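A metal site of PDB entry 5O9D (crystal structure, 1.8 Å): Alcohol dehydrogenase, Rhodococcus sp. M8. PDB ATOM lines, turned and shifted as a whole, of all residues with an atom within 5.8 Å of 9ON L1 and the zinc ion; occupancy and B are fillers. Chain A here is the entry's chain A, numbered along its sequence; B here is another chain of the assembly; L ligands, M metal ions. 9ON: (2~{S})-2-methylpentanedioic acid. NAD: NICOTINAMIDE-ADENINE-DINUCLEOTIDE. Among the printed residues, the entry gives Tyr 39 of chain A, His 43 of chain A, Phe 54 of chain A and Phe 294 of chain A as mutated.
Residues that only touch 9ON L1: Leu 119 (3.7 Å), Ile 271 (3.98 Å) and Phe 294 (3.5 Å).
Hydrophobic or aromatic side chains that line 9ON L1: His 62, Leu 119, Ile 271 and Phe 294.
Of the 18 residues printed, 7 come within 4 Å of 9ON L1.
The nearest printed residue that does not touch 9ON L1 is Val 44 (4.05 Å).
Ser 40 touches the zinc ion (OG to ZN, 3.8 Å).
Within 4 Å of the zinc ion: Cys 38, Ser 40, His 62 and Asp 153.
The nearest printed residue that does not touch the zinc ion is Arg 340 (4.7 Å).
The zinc ion is bound by the side-chain carboxylate of Asp 153, a ring nitrogen (NE2) of His 62, an oxygen (O9) of 9ON L1 and the side-chain sulfur of Cys 38.
The backbone carbonyl oxygen (O) of Ile 271 lies within hydrogen-bond range of an oxygen (O3D) of NAD L2, at 3.4 Å.
N of Ile 271 lies within hydrogen-bond range of O3D of NAD L2 (3.0 Å).
O2D of NAD L2 sits at hydrogen-bond distance from OG of Ser 40 (2.7 Å).
NE2 of His 43 sits at hydrogen-bond distance from O3D of NAD L2 (3.1 Å).
NH1 of Arg 340 lies within salt-bridge range of O1N of NAD L2, 2.7 Å away.
The backbone NH (N) of Leu 183 is in hydrogen-bond range of an oxygen (O2N) of NAD L2.
The side-chain hydroxyl (OG) of Ser 40 lies close to an oxygen (O9) of 9ON L1 (2.6 Å).
The backbone NH (N) of Tyr 39 lies within hydrogen-bond range of an oxygen (O1N) of NAD L2 (3.1 Å).
The backbone NH (N) of Cys 38 is in hydrogen-bond range of the side-chain carboxylate (OD2) of Asp 41.
NH2 of Arg 340 sits close to SG of Cys 38, at 3.4 Å.
The backbone carbonyl oxygen (O) of Ile 271 sits at hydrogen-bond distance from a ring nitrogen (NE2) of His 43 (3.1 Å).
The side-chain sulfur of Cys 38 lies close to the backbone NH of Ser 40.
ND1 of His 62 lies close to OD1 of Asp 41 (3.2 Å).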
ATOM      1  N   CYS A  38      13.915 -29.477   1.947  1.00  0.00           N
ATOM      2  CA  CYS A  38      13.023 -30.041   2.934  1.00  0.00           C
ATOM      3  C   CYS A  38      11.858 -30.718   2.212  1.00  0.00           C
ATOM      4  O   CYS A  38      11.378 -30.207   1.201  1.00  0.00           O
ATOM      5  CB  CYS A  38      12.496 -28.926   3.816  1.00  0.00           C
ATOM      6  SG  CYS A  38      11.314 -29.441   5.076  1.00  0.00           S
ATOM      7  N   TYR A  39      11.381 -31.829   2.736  1.00  0.00           N
ATOM      8  CA  TYR A  39      10.250 -32.508   2.109  1.00  0.00           C
ATOM      9  C   TYR A  39       8.999 -31.622   2.066  1.00  0.00           C
ATOM     10  O   TYR A  39       8.133 -31.827   1.223  1.00  0.00           O
ATOM     11  CB  TYR A  39       9.970 -33.859   2.740  1.00  0.00           C
ATOM     12  CG  TYR A  39       9.132 -34.743   1.878  1.00  0.00           C
ATOM     13  CD1 TYR A  39       9.714 -35.558   0.907  1.00  0.00           C
ATOM     14  CD2 TYR A  39       7.746 -34.762   1.997  1.00  0.00           C
ATOM     15  CE1 TYR A  39       8.942 -36.365   0.097  1.00  0.00           C
ATOM     16  CE2 TYR A  39       6.974 -35.556   1.198  1.00  0.00           C
ATOM     17  CZ  TYR A  39       7.573 -36.353   0.243  1.00  0.00           C
ATOM     18  OH  TYR A  39       6.783 -37.146  -0.539  1.00  0.00           O
ATOM     19  N   SER A  40       8.914 -30.604   2.938  1.00  0.00           N
ATOM     20  CA  SER A  40       7.812 -29.653   2.822  1.00  0.00           C
ATOM     21  C   SER A  40       7.759 -28.972   1.440  1.00  0.00           C
ATOM     22  O   SER A  40       6.686 -28.636   0.965  1.00  0.00           O
ATOM     23  CB  SER A  40       7.867 -28.602   3.921  1.00  0.00           C
ATOM     24  OG  SER A  40       7.581 -29.163   5.181  1.00  0.00           O
ATOM     25  N   ASP A  41       8.905 -28.799   0.803  1.00  0.00           N
ATOM     26  CA  ASP A  41       8.945 -28.263  -0.583  1.00  0.00           C
ATOM     27  C   ASP A  41       8.187 -29.176  -1.547  1.00  0.00           C
ATOM     28  O   ASP A  41       7.542 -28.698  -2.479  1.00  0.00           O
ATOM     29  CB  ASP A  41      10.380 -28.131  -1.068  1.00  0.00           C
ATOM     30  CG  ASP A  41      11.181 -27.128  -0.244  1.00  0.00           C
ATOM     31  OD1 ASP A  41      10.566 -26.185   0.316  1.00  0.00           O
ATOM     32  OD2 ASP A  41      12.428 -27.273  -0.157  1.00  0.00           O
ATOM     33  N   HIS A  43       5.576 -31.117  -0.587  1.00  0.00           N
ATOM     34  CA  HIS A  43       4.156 -30.818  -0.293  1.00  0.00           C
ATOM     35  C   HIS A  43       3.712 -29.558  -1.029  1.00  0.00           C
ATOM     36  O   HIS A  43       2.638 -29.555  -1.615  1.00  0.00           O
ATOM     37  CB  HIS A  43       3.874 -30.611   1.189  1.00  0.00           C
ATOM     38  CG  HIS A  43       4.121 -31.812   2.029  1.00  0.00           C
ATOM     39  ND1 HIS A  43       3.646 -33.056   1.702  1.00  0.00           N
ATOM     40  CD2 HIS A  43       4.797 -31.963   3.198  1.00  0.00           C
ATOM     41  CE1 HIS A  43       4.040 -33.930   2.621  1.00  0.00           C
ATOM     42  NE2 HIS A  43       4.736 -33.282   3.530  1.00  0.00           N
ATOM     43  N   VAL A  44       4.536 -28.528  -0.999  1.00  0.00           N
ATOM     44  CA  VAL A  44       4.197 -27.252  -1.645  1.00  0.00           C
ATOM     45  C   VAL A  44       4.003 -27.419  -3.149  1.00  0.00           C
ATOM     46  O   VAL A  44       2.992 -26.980  -3.698  1.00  0.00           O
ATOM     47  CB  VAL A  44       5.267 -26.173  -1.362  1.00  0.00           C
ATOM     48  CG1 VAL A  44       5.088 -24.937  -2.246  1.00  0.00           C
ATOM     49  CG2 VAL A  44       5.224 -25.790   0.102  1.00  0.00           C
ATOM     50  N   MET A  47       0.725 -29.169  -4.253  1.00  0.00           N
ATOM     51  CA  MET A  47      -0.555 -28.490  -4.055  1.00  0.00           C
ATOM     52  C   MET A  47      -1.199 -28.203  -5.403  1.00  0.00           C
ATOM     53  O   MET A  47      -0.512 -27.733  -6.319  1.00  0.00           O
ATOM     54  CB  MET A  47      -0.379 -27.168  -3.324  1.00  0.00           C
ATOM     55  CG  MET A  47      -0.004 -27.296  -1.867  1.00  0.00           C
ATOM     56  SD  MET A  47       0.327 -25.706  -1.102  1.00  0.00           S
ATOM     57  CE  MET A  47       0.721 -26.269   0.575  1.00  0.00           C
ATOM     58  N   PHE A  54       1.557 -19.294  -2.601  1.00  0.00           N
ATOM     59  CA  PHE A  54       2.853 -18.635  -2.403  1.00  0.00           C
ATOM     60  C   PHE A  54       3.343 -17.800  -3.572  1.00  0.00           C
ATOM     61  O   PHE A  54       4.429 -17.231  -3.492  1.00  0.00           O
ATOM     62  CB  PHE A  54       3.911 -19.661  -2.007  1.00  0.00           C
ATOM     63  CG  PHE A  54       3.632 -20.370  -0.709  1.00  0.00           C
ATOM     64  CD1 PHE A  54       2.912 -19.770   0.318  1.00  0.00           C
ATOM     65  CD2 PHE A  54       4.135 -21.630  -0.492  1.00  0.00           C
ATOM     66  CE1 PHE A  54       2.669 -20.438   1.508  1.00  0.00           C
ATOM     67  CE2 PHE A  54       3.892 -22.297   0.698  1.00  0.00           C
ATOM     68  CZ  PHE A  54       3.162 -21.697   1.698  1.00  0.00           C
ATOM     69  N   HIS A  62      13.846 -22.890   2.205  1.00  0.00           N
ATOM     70  CA  HIS A  62      13.617 -22.227   3.494  1.00  0.00           C
ATOM     71  C   HIS A  62      14.602 -22.659   4.572  1.00  0.00           C
ATOM     72  O   HIS A  62      14.393 -22.370   5.774  1.00  0.00           O
ATOM     73  CB  HIS A  62      12.176 -22.418   3.959  1.00  0.00           C
ATOM     74  CG  HIS A  62      11.762 -23.850   4.054  1.00  0.00           C
ATOM     75  ND1 HIS A  62      11.244 -24.547   2.975  1.00  0.00           N
ATOM     76  CD2 HIS A  62      11.749 -24.696   5.096  1.00  0.00           C
ATOM     77  CE1 HIS A  62      10.942 -25.778   3.372  1.00  0.00           C
ATOM     78  NE2 HIS A  62      11.210 -25.879   4.655  1.00  0.00           N
ATOM     79  N   GLU A  63      15.661 -23.348   4.155  1.00  0.00           N
ATOM     80  CA  GLU A  63      16.794 -23.698   4.990  1.00  0.00           C
ATOM     81  C   GLU A  63      18.010 -23.005   4.432  1.00  0.00           C
ATOM     82  O   GLU A  63      18.622 -23.502   3.508  1.00  0.00           O
ATOM     83  CB  GLU A  63      17.025 -25.215   5.003  1.00  0.00           C
ATOM     84  CG  GLU A  63      15.991 -26.018   5.771  1.00  0.00           C
ATOM     85  CD  GLU A  63      16.391 -27.490   5.969  1.00  0.00           C
ATOM     86  OE1 GLU A  63      17.221 -28.032   5.211  1.00  0.00           O
ATOM     87  OE2 GLU A  63      15.864 -28.128   6.900  1.00  0.00           O
ATOM     88  N   LEU A 119       8.772 -19.837   0.990  1.00  0.00           N
ATOM     89  CA  LEU A 119       7.388 -20.200   1.263  1.00  0.00           C
ATOM     90  C   LEU A 119       6.489 -18.953   1.164  1.00  0.00           C
ATOM     91  O   LEU A 119       5.615 -18.743   1.996  1.00  0.00           O
ATOM     92  CB  LEU A 119       7.282 -20.861   2.649  1.00  0.00           C
ATOM     93  CG  LEU A 119       8.123 -22.116   2.906  1.00  0.00           C
ATOM     94  CD1 LEU A 119       8.227 -22.459   4.392  1.00  0.00           C
ATOM     95  CD2 LEU A 119       7.549 -23.264   2.106  1.00  0.00           C
ATOM     96  N   ASP A 153      15.831 -25.947   9.860  1.00  0.00           N
ATOM     97  CA  ASP A 153      14.530 -26.568   9.856  1.00  0.00           C
ATOM     98  C   ASP A 153      14.588 -28.029  10.281  1.00  0.00           C
ATOM     99  O   ASP A 153      13.891 -28.418  11.233  1.00  0.00           O
ATOM    100  CB  ASP A 153      13.896 -26.381   8.502  1.00  0.00           C
ATOM    101  CG  ASP A 153      12.402 -26.626   8.508  1.00  0.00           C
ATOM    102  OD1 ASP A 153      11.733 -26.626   9.583  1.00  0.00           O
ATOM    103  OD2 ASP A 153      11.922 -26.793   7.402  1.00  0.00           O
ATOM    104  N   LEU A 183      14.568 -34.592   9.122  1.00  0.00           N
ATOM    105  CA  LEU A 183      14.235 -34.180  10.487  1.00  0.00           C
ATOM    106  C   LEU A 183      14.587 -35.284  11.482  1.00  0.00           C
ATOM    107  O   LEU A 183      15.212 -35.002  12.516  1.00  0.00           O
ATOM    108  CB  LEU A 183      12.760 -33.829  10.643  1.00  0.00           C
ATOM    109  CG  LEU A 183      12.411 -32.365  10.363  1.00  0.00           C
ATOM    110  CD1 LEU A 183      12.666 -31.974   8.900  1.00  0.00           C
ATOM    111  CD2 LEU A 183      10.962 -32.121  10.774  1.00  0.00           C
ATOM    112  N   ILE A 271       3.796 -34.110   8.063  1.00  0.00           N
ATOM    113  CA  ILE A 271       2.569 -33.608   7.454  1.00  0.00           C
ATOM    114  C   ILE A 271       2.113 -34.605   6.381  1.00  0.00           C
ATOM    115  O   ILE A 271       2.819 -34.876   5.395  1.00  0.00           O
ATOM    116  CB  ILE A 271       2.817 -32.214   6.835  1.00  0.00           C
ATOM    117  CG1 ILE A 271       3.262 -31.229   7.933  1.00  0.00           C
ATOM    118  CG2 ILE A 271       1.589 -31.699   6.099  1.00  0.00           C
ATOM    119  CD1 ILE A 271       3.927 -29.971   7.333  1.00  0.00           C
ATOM    120  N   PHE A 294       5.046 -26.486  15.167  1.00  0.00           N
ATOM    121  CA  PHE A 294       5.427 -25.824  13.928  1.00  0.00           C
ATOM    122  C   PHE A 294       6.731 -25.080  14.103  1.00  0.00           C
ATOM    123  O   PHE A 294       6.828 -24.191  14.951  1.00  0.00           O
ATOM    124  CB  PHE A 294       4.350 -24.868  13.464  1.00  0.00           C
ATOM    125  CG  PHE A 294       4.688 -24.168  12.176  1.00  0.00           C
ATOM    126  CD1 PHE A 294       4.682 -24.860  10.970  1.00  0.00           C
ATOM    127  CD2 PHE A 294       5.063 -22.835  12.180  1.00  0.00           C
ATOM    128  CE1 PHE A 294       5.009 -24.202   9.792  1.00  0.00           C
ATOM    129  CE2 PHE A 294       5.407 -22.174  11.007  1.00  0.00           C
ATOM    130  CZ  PHE A 294       5.391 -22.869   9.814  1.00  0.00           C
ATOM    131  N   ARG A 340      19.873 -35.203   4.614  1.00  0.00           N
ATOM    132  CA  ARG A 340      19.400 -33.944   4.036  1.00  0.00           C
ATOM    133  C   ARG A 340      20.138 -33.579   2.762  1.00  0.00           C
ATOM    134  O   ARG A 340      21.367 -33.599   2.719  1.00  0.00           O
ATOM    135  CB  ARG A 340      19.586 -32.809   5.048  1.00  0.00           C
ATOM    136  CG  ARG A 340      18.318 -32.346   5.684  1.00  0.00           C
ATOM    137  CD  ARG A 340      17.525 -31.491   4.714  1.00  0.00           C
ATOM    138  NE  ARG A 340      16.468 -30.768   5.385  1.00  0.00           N
ATOM    139  CZ  ARG A 340      15.241 -31.227   5.611  1.00  0.00           C
ATOM    140  NH1 ARG A 340      14.870 -32.442   5.248  1.00  0.00           N
ATOM    141  NH2 ARG A 340      14.373 -30.428   6.196  1.00  0.00           N
ATOM    142  N   PHE B 281      -2.607 -31.668  11.193  1.00  0.00           N
ATOM    143  CA  PHE B 281      -2.400 -30.438  10.437  1.00  0.00           C
ATOM    144  C   PHE B 281      -3.634 -30.040   9.681  1.00  0.00           C
ATOM    145  O   PHE B 281      -4.335 -30.903   9.163  1.00  0.00           O
ATOM    146  CB  PHE B 281      -1.189 -30.559   9.529  1.00  0.00           C
ATOM    147  CG  PHE B 281       0.096 -30.557  10.283  1.00  0.00           C
ATOM    148  CD1 PHE B 281       0.639 -29.361  10.745  1.00  0.00           C
ATOM    149  CD2 PHE B 281       0.699 -31.755  10.636  1.00  0.00           C
ATOM    150  CE1 PHE B 281       1.829 -29.357  11.470  1.00  0.00           C
ATOM    151  CE2 PHE B 281       1.889 -31.751  11.361  1.00  0.00           C
ATOM    152  CZ  PHE B 281       2.442 -30.556  11.787  1.00  0.00           C
ATOM    153  N   PHE B 286      -1.681 -24.704  14.838  1.00  0.00           N
ATOM    154  CA  PHE B 286      -0.318 -25.020  15.231  1.00  0.00           C
ATOM    155  C   PHE B 286      -0.108 -24.863  16.729  1.00  0.00           C
ATOM    156  O   PHE B 286      -0.584 -23.898  17.325  1.00  0.00           O
ATOM    157  CB  PHE B 286       0.701 -24.099  14.555  1.00  0.00           C
ATOM    158  CG  PHE B 286       0.765 -24.211  13.056  1.00  0.00           C
ATOM    159  CD1 PHE B 286       0.566 -25.414  12.398  1.00  0.00           C
ATOM    160  CD2 PHE B 286       1.117 -23.085  12.300  1.00  0.00           C
ATOM    161  CE1 PHE B 286       0.678 -25.506  11.031  1.00  0.00           C
ATOM    162  CE2 PHE B 286       1.226 -23.163  10.934  1.00  0.00           C
ATOM    163  CZ  PHE B 286       0.997 -24.382  10.287  1.00  0.00           C
HETATM  164  O12 9ON L   1       3.330 -26.036   7.326  1.00  0.00           O
HETATM  165  C7  9ON L   1       3.823 -25.369   6.386  1.00  0.00           C
HETATM  166  O10 9ON L   1       3.660 -24.145   6.249  1.00  0.00           O
HETATM  167  C4  9ON L   1       4.663 -26.111   5.389  1.00  0.00           C
HETATM  168  C5  9ON L   1       4.096 -25.889   3.990  1.00  0.00           C
HETATM  169  C3  9ON L   1       6.105 -25.601   5.533  1.00  0.00           C
HETATM  170  C2  9ON L   1       6.756 -26.099   6.822  1.00  0.00           C
HETATM  171  C1  9ON L   1       8.261 -26.160   6.692  1.00  0.00           C
HETATM  172  O8  9ON L   1       8.901 -25.116   6.937  1.00  0.00           O
HETATM  173  O9  9ON L   1       8.820 -27.227   6.362  1.00  0.00           O
HETATM  174  PA  NAD L   2      12.371 -36.918   4.413  1.00  0.00           P
HETATM  175  O1A NAD L   2      11.743 -37.341   3.102  1.00  0.00           O
HETATM  176  O2A NAD L   2      13.809 -36.498   4.494  1.00  0.00           O
HETATM  177  O5B NAD L   2      12.247 -38.164   5.394  1.00  0.00           O
HETATM  178  C5B NAD L   2      11.159 -39.087   5.405  1.00  0.00           C
HETATM  179  C4B NAD L   2      11.586 -40.268   6.266  1.00  0.00           C
HETATM  180  O4B NAD L   2      10.396 -40.888   6.731  1.00  0.00           O
HETATM  181  C3B NAD L   2      12.391 -41.320   5.499  1.00  0.00           C
HETATM  182  O3B NAD L   2      13.452 -41.867   6.303  1.00  0.00           O
HETATM  183  C2B NAD L   2      11.340 -42.373   5.156  1.00  0.00           C
HETATM  184  O2B NAD L   2      11.826 -43.716   4.996  1.00  0.00           O
HETATM  185  C1B NAD L   2      10.470 -42.277   6.398  1.00  0.00           C
HETATM  186  N9A NAD L   2       9.100 -42.800   6.271  1.00  0.00           N
HETATM  187  C8A NAD L   2       8.206 -42.539   5.297  1.00  0.00           C
HETATM  188  N7A NAD L   2       7.039 -43.176   5.553  1.00  0.00           N
HETATM  189  C5A NAD L   2       7.222 -43.854   6.709  1.00  0.00           C
HETATM  190  C6A NAD L   2       6.378 -44.713   7.557  1.00  0.00           C
HETATM  191  N6A NAD L   2       5.119 -44.987   7.172  1.00  0.00           N
HETATM  192  N1A NAD L   2       6.903 -45.204   8.691  1.00  0.00           N
HETATM  193  C2A NAD L   2       8.159 -44.917   9.078  1.00  0.00           C
HETATM  194  N3A NAD L   2       8.991 -44.132   8.359  1.00  0.00           N
HETATM  195  C4A NAD L   2       8.568 -43.590   7.180  1.00  0.00           C
HETATM  196  O3  NAD L   2      11.380 -35.855   5.055  1.00  0.00           O
HETATM  197  PN  NAD L   2      11.801 -34.619   5.995  1.00  0.00           P
HETATM  198  O1N NAD L   2      12.325 -33.474   5.169  1.00  0.00           O
HETATM  199  O2N NAD L   2      12.560 -35.161   7.183  1.00  0.00           O
HETATM  200  O5D NAD L   2      10.354 -34.178   6.482  1.00  0.00           O
HETATM  201  C5D NAD L   2       9.533 -35.079   7.227  1.00  0.00           C
HETATM  202  C4D NAD L   2       8.125 -34.509   7.394  1.00  0.00           C
HETATM  203  O4D NAD L   2       8.148 -33.404   8.314  1.00  0.00           O
HETATM  204  C3D NAD L   2       7.486 -33.994   6.111  1.00  0.00           C
HETATM  205  O3D NAD L   2       6.089 -34.300   6.081  1.00  0.00           O
HETATM  206  C2D NAD L   2       7.678 -32.504   6.223  1.00  0.00           C
HETATM  207  O2D NAD L   2       6.756 -31.737   5.457  1.00  0.00           O
HETATM  208  C1D NAD L   2       7.453 -32.305   7.706  1.00  0.00           C
HETATM  209  N1N NAD L   2       7.953 -31.065   8.279  1.00  0.00           N
HETATM  210  C2N NAD L   2       7.219 -30.505   9.237  1.00  0.00           C
HETATM  211  C3N NAD L   2       7.623 -29.338   9.875  1.00  0.00           C
HETATM  212  C7N NAD L   2       6.818 -28.705  10.954  1.00  0.00           C
HETATM  213  O7N NAD L   2       7.117 -27.574  11.331  1.00  0.00           O
HETATM  214  N7N NAD L   2       5.830 -29.364  11.570  1.00  0.00           N
HETATM  215  C4N NAD L   2       8.860 -28.774   9.498  1.00  0.00           C
HETATM  216  C5N NAD L   2       9.636 -29.395   8.524  1.00  0.00           C
HETATM  217  C6N NAD L   2       9.168 -30.553   7.931  1.00  0.00           C
HETATM  218 ZN    ZN M   1      10.832 -27.415   5.944  1.00  0.00          ZN
